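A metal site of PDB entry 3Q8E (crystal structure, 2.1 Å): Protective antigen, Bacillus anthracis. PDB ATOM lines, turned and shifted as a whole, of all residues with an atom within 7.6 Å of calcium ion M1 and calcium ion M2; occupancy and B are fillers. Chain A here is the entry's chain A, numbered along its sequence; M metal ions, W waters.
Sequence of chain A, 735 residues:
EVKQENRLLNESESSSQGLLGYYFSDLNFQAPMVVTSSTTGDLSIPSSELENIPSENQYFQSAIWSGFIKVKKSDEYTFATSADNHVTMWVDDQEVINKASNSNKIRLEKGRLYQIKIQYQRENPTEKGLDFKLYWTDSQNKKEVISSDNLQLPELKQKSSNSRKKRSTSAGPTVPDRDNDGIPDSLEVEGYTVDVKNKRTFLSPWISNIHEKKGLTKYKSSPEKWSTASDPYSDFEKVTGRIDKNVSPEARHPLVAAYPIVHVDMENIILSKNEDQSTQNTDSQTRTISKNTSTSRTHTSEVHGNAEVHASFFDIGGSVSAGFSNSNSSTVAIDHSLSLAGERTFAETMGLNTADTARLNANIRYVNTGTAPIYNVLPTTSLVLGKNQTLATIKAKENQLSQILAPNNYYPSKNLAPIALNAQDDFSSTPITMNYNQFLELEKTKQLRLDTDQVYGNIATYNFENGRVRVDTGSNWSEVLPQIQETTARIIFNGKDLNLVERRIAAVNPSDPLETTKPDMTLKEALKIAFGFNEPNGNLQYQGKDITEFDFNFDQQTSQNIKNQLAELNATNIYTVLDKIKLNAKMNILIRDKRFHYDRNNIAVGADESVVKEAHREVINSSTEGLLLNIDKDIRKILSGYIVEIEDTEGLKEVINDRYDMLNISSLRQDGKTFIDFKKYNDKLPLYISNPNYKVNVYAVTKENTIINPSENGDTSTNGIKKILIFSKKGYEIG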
ATOM      1  N   TYR A  22     -27.687  -9.771 -17.830  1.00  0.00           N
ATOM      2  CA  TYR A  22     -28.968  -9.539 -18.458  1.00  0.00           C
ATOM      3  C   TYR A  22     -29.732  -8.574 -17.567  1.00  0.00           C
ATOM      4  O   TYR A  22     -30.028  -8.882 -16.434  1.00  0.00           O
ATOM      5  CB  TYR A  22     -29.751 -10.849 -18.610  1.00  0.00           C
ATOM      6  CG  TYR A  22     -29.025 -11.854 -19.489  1.00  0.00           C
ATOM      7  CD1 TYR A  22     -28.384 -12.954 -18.949  1.00  0.00           C
ATOM      8  CD2 TYR A  22     -28.964 -11.676 -20.860  1.00  0.00           C
ATOM      9  CE1 TYR A  22     -27.706 -13.850 -19.762  1.00  0.00           C
ATOM     10  CE2 TYR A  22     -28.308 -12.554 -21.665  1.00  0.00           C
ATOM     11  CZ  TYR A  22     -27.685 -13.642 -21.130  1.00  0.00           C
ATOM     12  OH  TYR A  22     -27.045 -14.494 -21.963  1.00  0.00           O
ATOM     13  N   PRO A 176     -34.179 -17.465 -21.126  1.00  0.00           N
ATOM     14  CA  PRO A 176     -34.332 -18.368 -22.259  1.00  0.00           C
ATOM     15  C   PRO A 176     -33.292 -18.093 -23.362  1.00  0.00           C
ATOM     16  O   PRO A 176     -33.206 -16.987 -23.883  1.00  0.00           O
ATOM     17  CB  PRO A 176     -35.763 -18.090 -22.748  1.00  0.00           C
ATOM     18  CG  PRO A 176     -36.386 -17.166 -21.681  1.00  0.00           C
ATOM     19  CD  PRO A 176     -35.217 -16.436 -21.083  1.00  0.00           C
ATOM     20  N   ASP A 177     -32.513 -19.128 -23.641  1.00  0.00           N
ATOM     21  CA  ASP A 177     -31.375 -19.092 -24.549  1.00  0.00           C
ATOM     22  C   ASP A 177     -31.199 -20.508 -25.097  1.00  0.00           C
ATOM     23  O   ASP A 177     -30.273 -21.215 -24.720  1.00  0.00           O
ATOM     24  CB  ASP A 177     -30.107 -18.645 -23.806  1.00  0.00           C
ATOM     25  CG  ASP A 177     -28.919 -18.418 -24.769  1.00  0.00           C
ATOM     26  OD1 ASP A 177     -29.121 -18.416 -25.990  1.00  0.00           O
ATOM     27  OD2 ASP A 177     -27.778 -18.237 -24.314  1.00  0.00           O
ATOM     28  N   ARG A 178     -32.101 -20.930 -25.974  1.00  0.00           N
ATOM     29  CA  ARG A 178     -32.172 -22.320 -26.417  1.00  0.00           C
ATOM     30  C   ARG A 178     -30.894 -22.817 -27.123  1.00  0.00           C
ATOM     31  O   ARG A 178     -30.583 -23.994 -27.069  1.00  0.00           O
ATOM     32  CB  ARG A 178     -33.375 -22.506 -27.353  1.00  0.00           C
ATOM     33  CG  ARG A 178     -34.723 -22.098 -26.733  1.00  0.00           C
ATOM     34  CD  ARG A 178     -35.820 -21.779 -27.772  1.00  0.00           C
ATOM     35  NE  ARG A 178     -36.564 -22.961 -28.190  1.00  0.00           N
ATOM     36  CZ  ARG A 178     -37.338 -23.685 -27.389  1.00  0.00           C
ATOM     37  NH1 ARG A 178     -37.457 -23.365 -26.105  1.00  0.00           N
ATOM     38  NH2 ARG A 178     -37.985 -24.748 -27.865  1.00  0.00           N
ATOM     39  N   ASP A 179     -30.163 -21.948 -27.821  1.00  0.00           N
ATOM     40  CA  ASP A 179     -28.935 -22.416 -28.534  1.00  0.00           C
ATOM     41  C   ASP A 179     -27.662 -22.089 -27.770  1.00  0.00           C
ATOM     42  O   ASP A 179     -26.559 -22.327 -28.249  1.00  0.00           O
ATOM     43  CB  ASP A 179     -28.833 -21.784 -29.923  1.00  0.00           C
ATOM     44  CG  ASP A 179     -28.959 -20.286 -29.855  1.00  0.00           C
ATOM     45  OD1 ASP A 179     -28.597 -19.685 -28.830  1.00  0.00           O
ATOM     46  OD2 ASP A 179     -29.467 -19.699 -30.816  1.00  0.00           O
ATOM     47  N   ASN A 180     -27.814 -21.506 -26.591  1.00  0.00           N
ATOM     48  CA  ASN A 180     -26.682 -21.168 -25.757  1.00  0.00           C
ATOM     49  C   ASN A 180     -25.655 -20.228 -26.407  1.00  0.00           C
ATOM     50  O   ASN A 180     -24.465 -20.329 -26.111  1.00  0.00           O
ATOM     51  CB  ASN A 180     -25.976 -22.445 -25.289  1.00  0.00           C
ATOM     52  CG  ASN A 180     -25.157 -22.234 -24.026  1.00  0.00           C
ATOM     53  OD1 ASN A 180     -25.594 -21.545 -23.113  1.00  0.00           O
ATOM     54  ND2 ASN A 180     -23.952 -22.774 -23.976  1.00  0.00           N
ATOM     55  N   ASP A 181     -26.065 -19.311 -27.295  1.00  0.00           N
ATOM     56  CA  ASP A 181     -25.047 -18.391 -27.809  1.00  0.00           C
ATOM     57  C   ASP A 181     -24.905 -17.201 -26.872  1.00  0.00           C
ATOM     58  O   ASP A 181     -23.932 -16.455 -26.926  1.00  0.00           O
ATOM     59  CB  ASP A 181     -25.273 -17.969 -29.282  1.00  0.00           C
ATOM     60  CG  ASP A 181     -26.637 -17.391 -29.529  1.00  0.00           C
ATOM     61  OD1 ASP A 181     -27.230 -16.823 -28.592  1.00  0.00           O
ATOM     62  OD2 ASP A 181     -27.110 -17.509 -30.659  1.00  0.00           O
ATOM     63  N   GLY A 182     -25.859 -17.054 -25.948  1.00  0.00           N
ATOM     64  CA  GLY A 182     -25.828 -15.944 -25.024  1.00  0.00           C
ATOM     65  C   GLY A 182     -26.827 -14.825 -25.326  1.00  0.00           C
ATOM     66  O   GLY A 182     -27.033 -13.942 -24.508  1.00  0.00           O
ATOM     67  N   ILE A 183     -27.425 -14.819 -26.515  1.00  0.00           N
ATOM     68  CA  ILE A 183     -28.442 -13.823 -26.851  1.00  0.00           C
ATOM     69  C   ILE A 183     -29.788 -14.472 -26.568  1.00  0.00           C
ATOM     70  O   ILE A 183     -30.068 -15.523 -27.120  1.00  0.00           O
ATOM     71  CB  ILE A 183     -28.403 -13.430 -28.339  1.00  0.00           C
ATOM     72  CG1 ILE A 183     -26.986 -12.967 -28.746  1.00  0.00           C
ATOM     73  CG2 ILE A 183     -29.467 -12.346 -28.597  1.00  0.00           C
ATOM     74  CD1 ILE A 183     -26.826 -12.677 -30.204  1.00  0.00           C
ATOM     75  N   PRO A 184     -30.620 -13.868 -25.707  1.00  0.00           N
ATOM     76  CA  PRO A 184     -31.929 -14.417 -25.328  1.00  0.00           C
ATOM     77  C   PRO A 184     -32.853 -14.656 -26.530  1.00  0.00           C
ATOM     78  O   PRO A 184     -32.808 -13.871 -27.475  1.00  0.00           O
ATOM     79  CB  PRO A 184     -32.515 -13.327 -24.406  1.00  0.00           C
ATOM     80  CG  PRO A 184     -31.328 -12.617 -23.850  1.00  0.00           C
ATOM     81  CD  PRO A 184     -30.272 -12.660 -24.931  1.00  0.00           C
ATOM     82  N   ASP A 185     -33.647 -15.721 -26.516  1.00  0.00           N
ATOM     83  CA  ASP A 185     -34.469 -16.080 -27.667  1.00  0.00           C
ATOM     84  C   ASP A 185     -35.223 -14.876 -28.226  1.00  0.00           C
ATOM     85  O   ASP A 185     -35.312 -14.694 -29.450  1.00  0.00           O
ATOM     86  CB  ASP A 185     -35.511 -17.129 -27.314  1.00  0.00           C
ATOM     87  CG  ASP A 185     -34.936 -18.386 -26.719  1.00  0.00           C
ATOM     88  OD1 ASP A 185     -33.698 -18.611 -26.785  1.00  0.00           O
ATOM     89  OD2 ASP A 185     -35.746 -19.170 -26.155  1.00  0.00           O
ATOM     90  N   SER A 186     -35.785 -14.076 -27.330  1.00  0.00           N
ATOM     91  CA  SER A 186     -36.748 -13.046 -27.721  1.00  0.00           C
ATOM     92  C   SER A 186     -36.078 -11.892 -28.434  1.00  0.00           C
ATOM     93  O   SER A 186     -36.676 -11.280 -29.326  1.00  0.00           O
ATOM     94  CB  SER A 186     -37.541 -12.520 -26.489  1.00  0.00           C
ATOM     95  OG  SER A 186     -36.694 -11.876 -25.555  1.00  0.00           O
ATOM     96  N   GLU A 188     -33.292 -12.336 -30.253  1.00  0.00           N
ATOM     97  CA  GLU A 188     -32.902 -12.890 -31.555  1.00  0.00           C
ATOM     98  C   GLU A 188     -34.088 -12.896 -32.524  1.00  0.00           C
ATOM     99  O   GLU A 188     -33.951 -12.654 -33.733  1.00  0.00           O
ATOM    100  CB  GLU A 188     -32.374 -14.313 -31.385  1.00  0.00           C
ATOM    101  CG  GLU A 188     -31.013 -14.383 -30.710  1.00  0.00           C
ATOM    102  CD  GLU A 188     -30.281 -15.640 -31.067  1.00  0.00           C
ATOM    103  OE1 GLU A 188     -30.376 -16.592 -30.300  1.00  0.00           O
ATOM    104  OE2 GLU A 188     -29.627 -15.710 -32.142  1.00  0.00           O
ATOM    105  N   TYR A 192     -32.438  -6.946 -32.612  1.00  0.00           N
ATOM    106  CA  TYR A 192     -31.553  -6.304 -31.666  1.00  0.00           C
ATOM    107  C   TYR A 192     -30.499  -5.454 -32.357  1.00  0.00           C
ATOM    108  O   TYR A 192     -30.245  -5.582 -33.560  1.00  0.00           O
ATOM    109  CB  TYR A 192     -30.862  -7.339 -30.786  1.00  0.00           C
ATOM    110  CG  TYR A 192     -30.081  -8.440 -31.499  1.00  0.00           C
ATOM    111  CD1 TYR A 192     -30.743  -9.515 -32.066  1.00  0.00           C
ATOM    112  CD2 TYR A 192     -28.684  -8.414 -31.554  1.00  0.00           C
ATOM    113  CE1 TYR A 192     -30.036 -10.532 -32.715  1.00  0.00           C
ATOM    114  CE2 TYR A 192     -27.969  -9.431 -32.210  1.00  0.00           C
ATOM    115  CZ  TYR A 192     -28.662 -10.488 -32.779  1.00  0.00           C
ATOM    116  OH  TYR A 192     -27.994 -11.510 -33.411  1.00  0.00           O
ATOM    117  N   SER A 221     -31.698 -13.090 -35.741  1.00  0.00           N
ATOM    118  CA  SER A 221     -30.990 -14.366 -35.832  1.00  0.00           C
ATOM    119  C   SER A 221     -31.855 -15.514 -35.299  1.00  0.00           C
ATOM    120  O   SER A 221     -32.888 -15.278 -34.671  1.00  0.00           O
ATOM    121  CB  SER A 221     -29.628 -14.271 -35.134  1.00  0.00           C
ATOM    122  OG  SER A 221     -29.682 -13.600 -33.884  1.00  0.00           O
ATOM    123  N   SER A 222     -31.493 -16.750 -35.610  1.00  0.00           N
ATOM    124  CA  SER A 222     -32.269 -17.886 -35.083  1.00  0.00           C
ATOM    125  C   SER A 222     -31.929 -18.157 -33.630  1.00  0.00           C
ATOM    126  O   SER A 222     -30.756 -18.346 -33.305  1.00  0.00           O
ATOM    127  CB  SER A 222     -31.993 -19.172 -35.847  1.00  0.00           C
ATOM    128  OG  SER A 222     -32.613 -20.255 -35.161  1.00  0.00           O
ATOM    129  N   PRO A 223     -32.970 -18.224 -32.768  1.00  0.00           N
ATOM    130  CA  PRO A 223     -32.796 -18.539 -31.322  1.00  0.00           C
ATOM    131  C   PRO A 223     -32.437 -19.998 -31.088  1.00  0.00           C
ATOM    132  O   PRO A 223     -32.110 -20.363 -29.956  1.00  0.00           O
ATOM    133  CB  PRO A 223     -34.177 -18.243 -30.722  1.00  0.00           C
ATOM    134  CG  PRO A 223     -35.151 -18.516 -31.835  1.00  0.00           C
ATOM    135  CD  PRO A 223     -34.393 -18.120 -33.152  1.00  0.00           C
ATOM    136  N   GLU A 224     -32.478 -20.805 -32.134  1.00  0.00           N
ATOM    137  CA  GLU A 224     -32.154 -22.223 -32.095  1.00  0.00           C
ATOM    138  C   GLU A 224     -30.870 -22.621 -32.842  1.00  0.00           C
ATOM    139  O   GLU A 224     -30.555 -23.807 -32.916  1.00  0.00           O
ATOM    140  CB  GLU A 224     -33.312 -22.980 -32.700  1.00  0.00           C
ATOM    141  CG  GLU A 224     -34.657 -22.425 -32.191  1.00  0.00           C
ATOM    142  CD  GLU A 224     -35.637 -23.492 -31.757  1.00  0.00           C
ATOM    143  OE1 GLU A 224     -36.622 -23.147 -31.035  1.00  0.00           O
ATOM    144  OE2 GLU A 224     -35.435 -24.665 -32.144  1.00  0.00           O
ATOM    145  N   LYS A 225     -30.171 -21.653 -33.428  1.00  0.00           N
ATOM    146  CA  LYS A 225     -28.882 -21.897 -34.076  1.00  0.00           C
ATOM    147  C   LYS A 225     -27.798 -21.077 -33.395  1.00  0.00           C
ATOM    148  O   LYS A 225     -27.802 -19.844 -33.467  1.00  0.00           O
ATOM    149  CB  LYS A 225     -29.003 -21.504 -35.544  1.00  0.00           C
ATOM    150  CG  LYS A 225     -30.025 -22.346 -36.278  1.00  0.00           C
ATOM    151  CD  LYS A 225     -29.909 -22.179 -37.814  1.00  0.00           C
ATOM    152  CE  LYS A 225     -28.895 -23.151 -38.363  1.00  0.00           C
ATOM    153  NZ  LYS A 225     -28.372 -22.636 -39.609  1.00  0.00           N
ATOM    154  N   TRP A 226     -26.871 -21.749 -32.717  1.00  0.00           N
ATOM    155  CA  TRP A 226     -25.757 -21.068 -32.080  1.00  0.00           C
ATOM    156  C   TRP A 226     -25.047 -20.159 -33.120  1.00  0.00           C
ATOM    157  O   TRP A 226     -24.774 -19.001 -32.828  1.00  0.00           O
ATOM    158  CB  TRP A 226     -24.822 -22.132 -31.457  1.00  0.00           C
ATOM    159  CG  TRP A 226     -23.589 -21.643 -30.834  1.00  0.00           C
ATOM    160  CD1 TRP A 226     -23.426 -21.256 -29.548  1.00  0.00           C
ATOM    161  CD2 TRP A 226     -22.287 -21.550 -31.456  1.00  0.00           C
ATOM    162  NE1 TRP A 226     -22.117 -20.908 -29.319  1.00  0.00           N
ATOM    163  CE2 TRP A 226     -21.397 -21.070 -30.481  1.00  0.00           C
ATOM    164  CE3 TRP A 226     -21.806 -21.791 -32.754  1.00  0.00           C
ATOM    165  CZ2 TRP A 226     -20.039 -20.847 -30.731  1.00  0.00           C
ATOM    166  CZ3 TRP A 226     -20.447 -21.561 -33.016  1.00  0.00           C
ATOM    167  CH2 TRP A 226     -19.574 -21.097 -32.003  1.00  0.00           C
ATOM    168  N   SER A 227     -24.805 -20.666 -34.324  1.00  0.00           N
ATOM    169  CA  SER A 227     -24.423 -19.812 -35.472  1.00  0.00           C
ATOM    170  C   SER A 227     -25.553 -19.896 -36.479  1.00  0.00           C
ATOM    171  O   SER A 227     -25.836 -20.968 -37.036  1.00  0.00           O
ATOM    172  CB  SER A 227     -23.108 -20.274 -36.120  1.00  0.00           C
ATOM    173  OG  SER A 227     -22.830 -19.513 -37.304  1.00  0.00           O
ATOM    174  N   THR A 228     -26.225 -18.780 -36.724  1.00  0.00           N
ATOM    175  CA  THR A 228     -27.387 -18.794 -37.579  1.00  0.00           C
ATOM    176  C   THR A 228     -26.971 -19.098 -39.029  1.00  0.00           C
ATOM    177  O   THR A 228     -27.703 -19.757 -39.766  1.00  0.00           O
ATOM    178  CB  THR A 228     -28.165 -17.484 -37.428  1.00  0.00           C
ATOM    179  OG1 THR A 228     -28.742 -17.440 -36.110  1.00  0.00           O
ATOM    180  CG2 THR A 228     -29.292 -17.412 -38.500  1.00  0.00           C
ATOM    181  N   SER A 234     -20.281 -17.880 -33.217  1.00  0.00           N
ATOM    182  CA  SER A 234     -21.645 -17.799 -32.699  1.00  0.00           C
ATOM    183  C   SER A 234     -22.234 -16.408 -33.012  1.00  0.00           C
ATOM    184  O   SER A 234     -21.492 -15.426 -33.197  1.00  0.00           O
ATOM    185  CB  SER A 234     -21.670 -18.018 -31.191  1.00  0.00           C
ATOM    186  OG  SER A 234     -21.652 -16.780 -30.514  1.00  0.00           O
ATOM    187  N   ASP A 235     -23.553 -16.325 -33.006  1.00  0.00           N
ATOM    188  CA  ASP A 235     -24.235 -15.054 -33.302  1.00  0.00           C
ATOM    189  C   ASP A 235     -23.793 -13.987 -32.323  1.00  0.00           C
ATOM    190  O   ASP A 235     -23.602 -12.834 -32.696  1.00  0.00           O
ATOM    191  CB  ASP A 235     -25.747 -15.246 -33.244  1.00  0.00           C
ATOM    192  CG  ASP A 235     -26.230 -16.228 -34.285  1.00  0.00           C
ATOM    193  OD1 ASP A 235     -25.548 -16.407 -35.314  1.00  0.00           O
ATOM    194  OD2 ASP A 235     -27.293 -16.812 -34.117  1.00  0.00           O
ATOM    195  N   PHE A 236     -23.594 -14.395 -31.068  1.00  0.00           N
ATOM    196  CA  PHE A 236     -23.094 -13.483 -30.032  1.00  0.00           C
ATOM    197  C   PHE A 236     -21.607 -13.099 -30.269  1.00  0.00           C
ATOM    198  O   PHE A 236     -21.223 -11.944 -30.154  1.00  0.00           O
ATOM    199  CB  PHE A 236     -23.293 -14.137 -28.676  1.00  0.00           C
ATOM    200  CG  PHE A 236     -22.889 -13.306 -27.502  1.00  0.00           C
ATOM    201  CD1 PHE A 236     -23.699 -12.257 -27.063  1.00  0.00           C
ATOM    202  CD2 PHE A 236     -21.729 -13.609 -26.792  1.00  0.00           C
ATOM    203  CE1 PHE A 236     -23.351 -11.492 -25.943  1.00  0.00           C
ATOM    204  CE2 PHE A 236     -21.370 -12.857 -25.662  1.00  0.00           C
ATOM    205  CZ  PHE A 236     -22.184 -11.795 -25.240  1.00  0.00           C
ATOM    206  N   PRO A 254     -24.794 -11.919 -38.114  1.00  0.00           N
ATOM    207  CA  PRO A 254     -25.227 -13.293 -37.853  1.00  0.00           C
ATOM    208  C   PRO A 254     -25.797 -14.005 -39.087  1.00  0.00           C
ATOM    209  O   PRO A 254     -25.745 -15.235 -39.156  1.00  0.00           O
ATOM    210  CB  PRO A 254     -26.295 -13.129 -36.770  1.00  0.00           C
ATOM    211  CG  PRO A 254     -25.923 -11.899 -36.068  1.00  0.00           C
ATOM    212  CD  PRO A 254     -25.333 -10.978 -37.117  1.00  0.00           C
HETATM  213 CA    CA M   1     -29.522 -17.486 -28.253  1.00  0.00          CA
HETATM  214 CA    CA M   2     -28.648 -17.842 -32.269  1.00  0.00          CA
HETATM  215  O   HOH W   1     -31.676 -18.560 -28.259  1.00  0.00           O
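Water W1 lies within hydrogen-bond range of OD1 of Asp 185 (2.5 Å), O of Pro 223 (2.5 Å) and N of Arg 178 (3.3 Å).
Five residues have an atom within 4 Å of calcium ion M1: Asp 177, Asp 179, Asp 181, Ile 183 and Glu 188.
The nearest printed residue that does not touch calcium ion M1 is Pro 223 (4.2 Å).
OG1 of Thr 228 touches calcium ion M2, at 3.9 Å.
Seven residues have an atom within 4 Å of calcium ion M2: Asp 179, Asp 181, Glu 188, Ser 222, Lys 225, Thr 228 and Asp 235.
The nearest printed residue that does not touch calcium ion M2 is Trp 226 (4.1 Å).
The side-chain carboxylate (OD2) of Asp 181 is bound to calcium ion M2, 2.3 Å away.
Calcium ion M2 is bound by the side-chain carboxylate (OE2) of Glu 188, 2.3 Å away.
O of Ser 222 binds calcium ion M2 (2.4 Å).
O of Lys 225 binds calcium ion M2 (2.5 Å).
OD2 of Asp 179 binds calcium ion M2 (2.5 Å).
Calcium ion M2 is bound by the side-chain carboxylate (OD2) of Asp 235 (2.5 Å).
Calcium ion M2 has six donor atoms within binding distance.
Slightly farther from calcium ion M2 lies the side-chain carboxylate (OE1) of Glu 188 (2.9 Å).
O of Ile 183 is bound to calcium ion M1, 2.3 Å away.
Calcium ion M1 is bound by the side-chain carboxylate (OE1) of Glu 188, 2.4 Å away.
Water W1 binds calcium ion M1, 2.4 Å away.
Calcium ion M1 is bound by OD1 of Asp 181 (2.4 Å).
Calcium ion M1 is bound by OD1 of Asp 179, 2.5 Å away.
Calcium ion M1 is bound by the side-chain carboxylate (OD1) of Asp 177 (2.5 Å).
Calcium ion M1 has six donor atoms within binding distance.
OG of Ser 222 lies within hydrogen-bond range of N of Lys 225 (3.3 Å).
The side-chain hydroxyl (OG) of Ser 222 is in hydrogen-bond range of the backbone NH (N) of Glu 224 (3.1 Å).
O of Pro 223 sits close to N of Asp 179.
The side-chain carboxylate (OD2) of Asp 179 lies close to the backbone NH (N) of Glu 224, 3.5 Å away.
The backbone NH of Gly 182 is in hydrogen-bond range of the side-chain carboxylate of Asp 177 (2.8 Å).
N of Asp 177 lies close to OD1 of Asp 185 (3.4 Å).
NZ of Lys 225 is in hydrogen-bond range of O of Thr 228 (3.0 Å).
The backbone NH (N) of Thr 228 lies within hydrogen-bond range of the side-chain carboxylate (OD1) of Asp 235 (2.8 Å).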
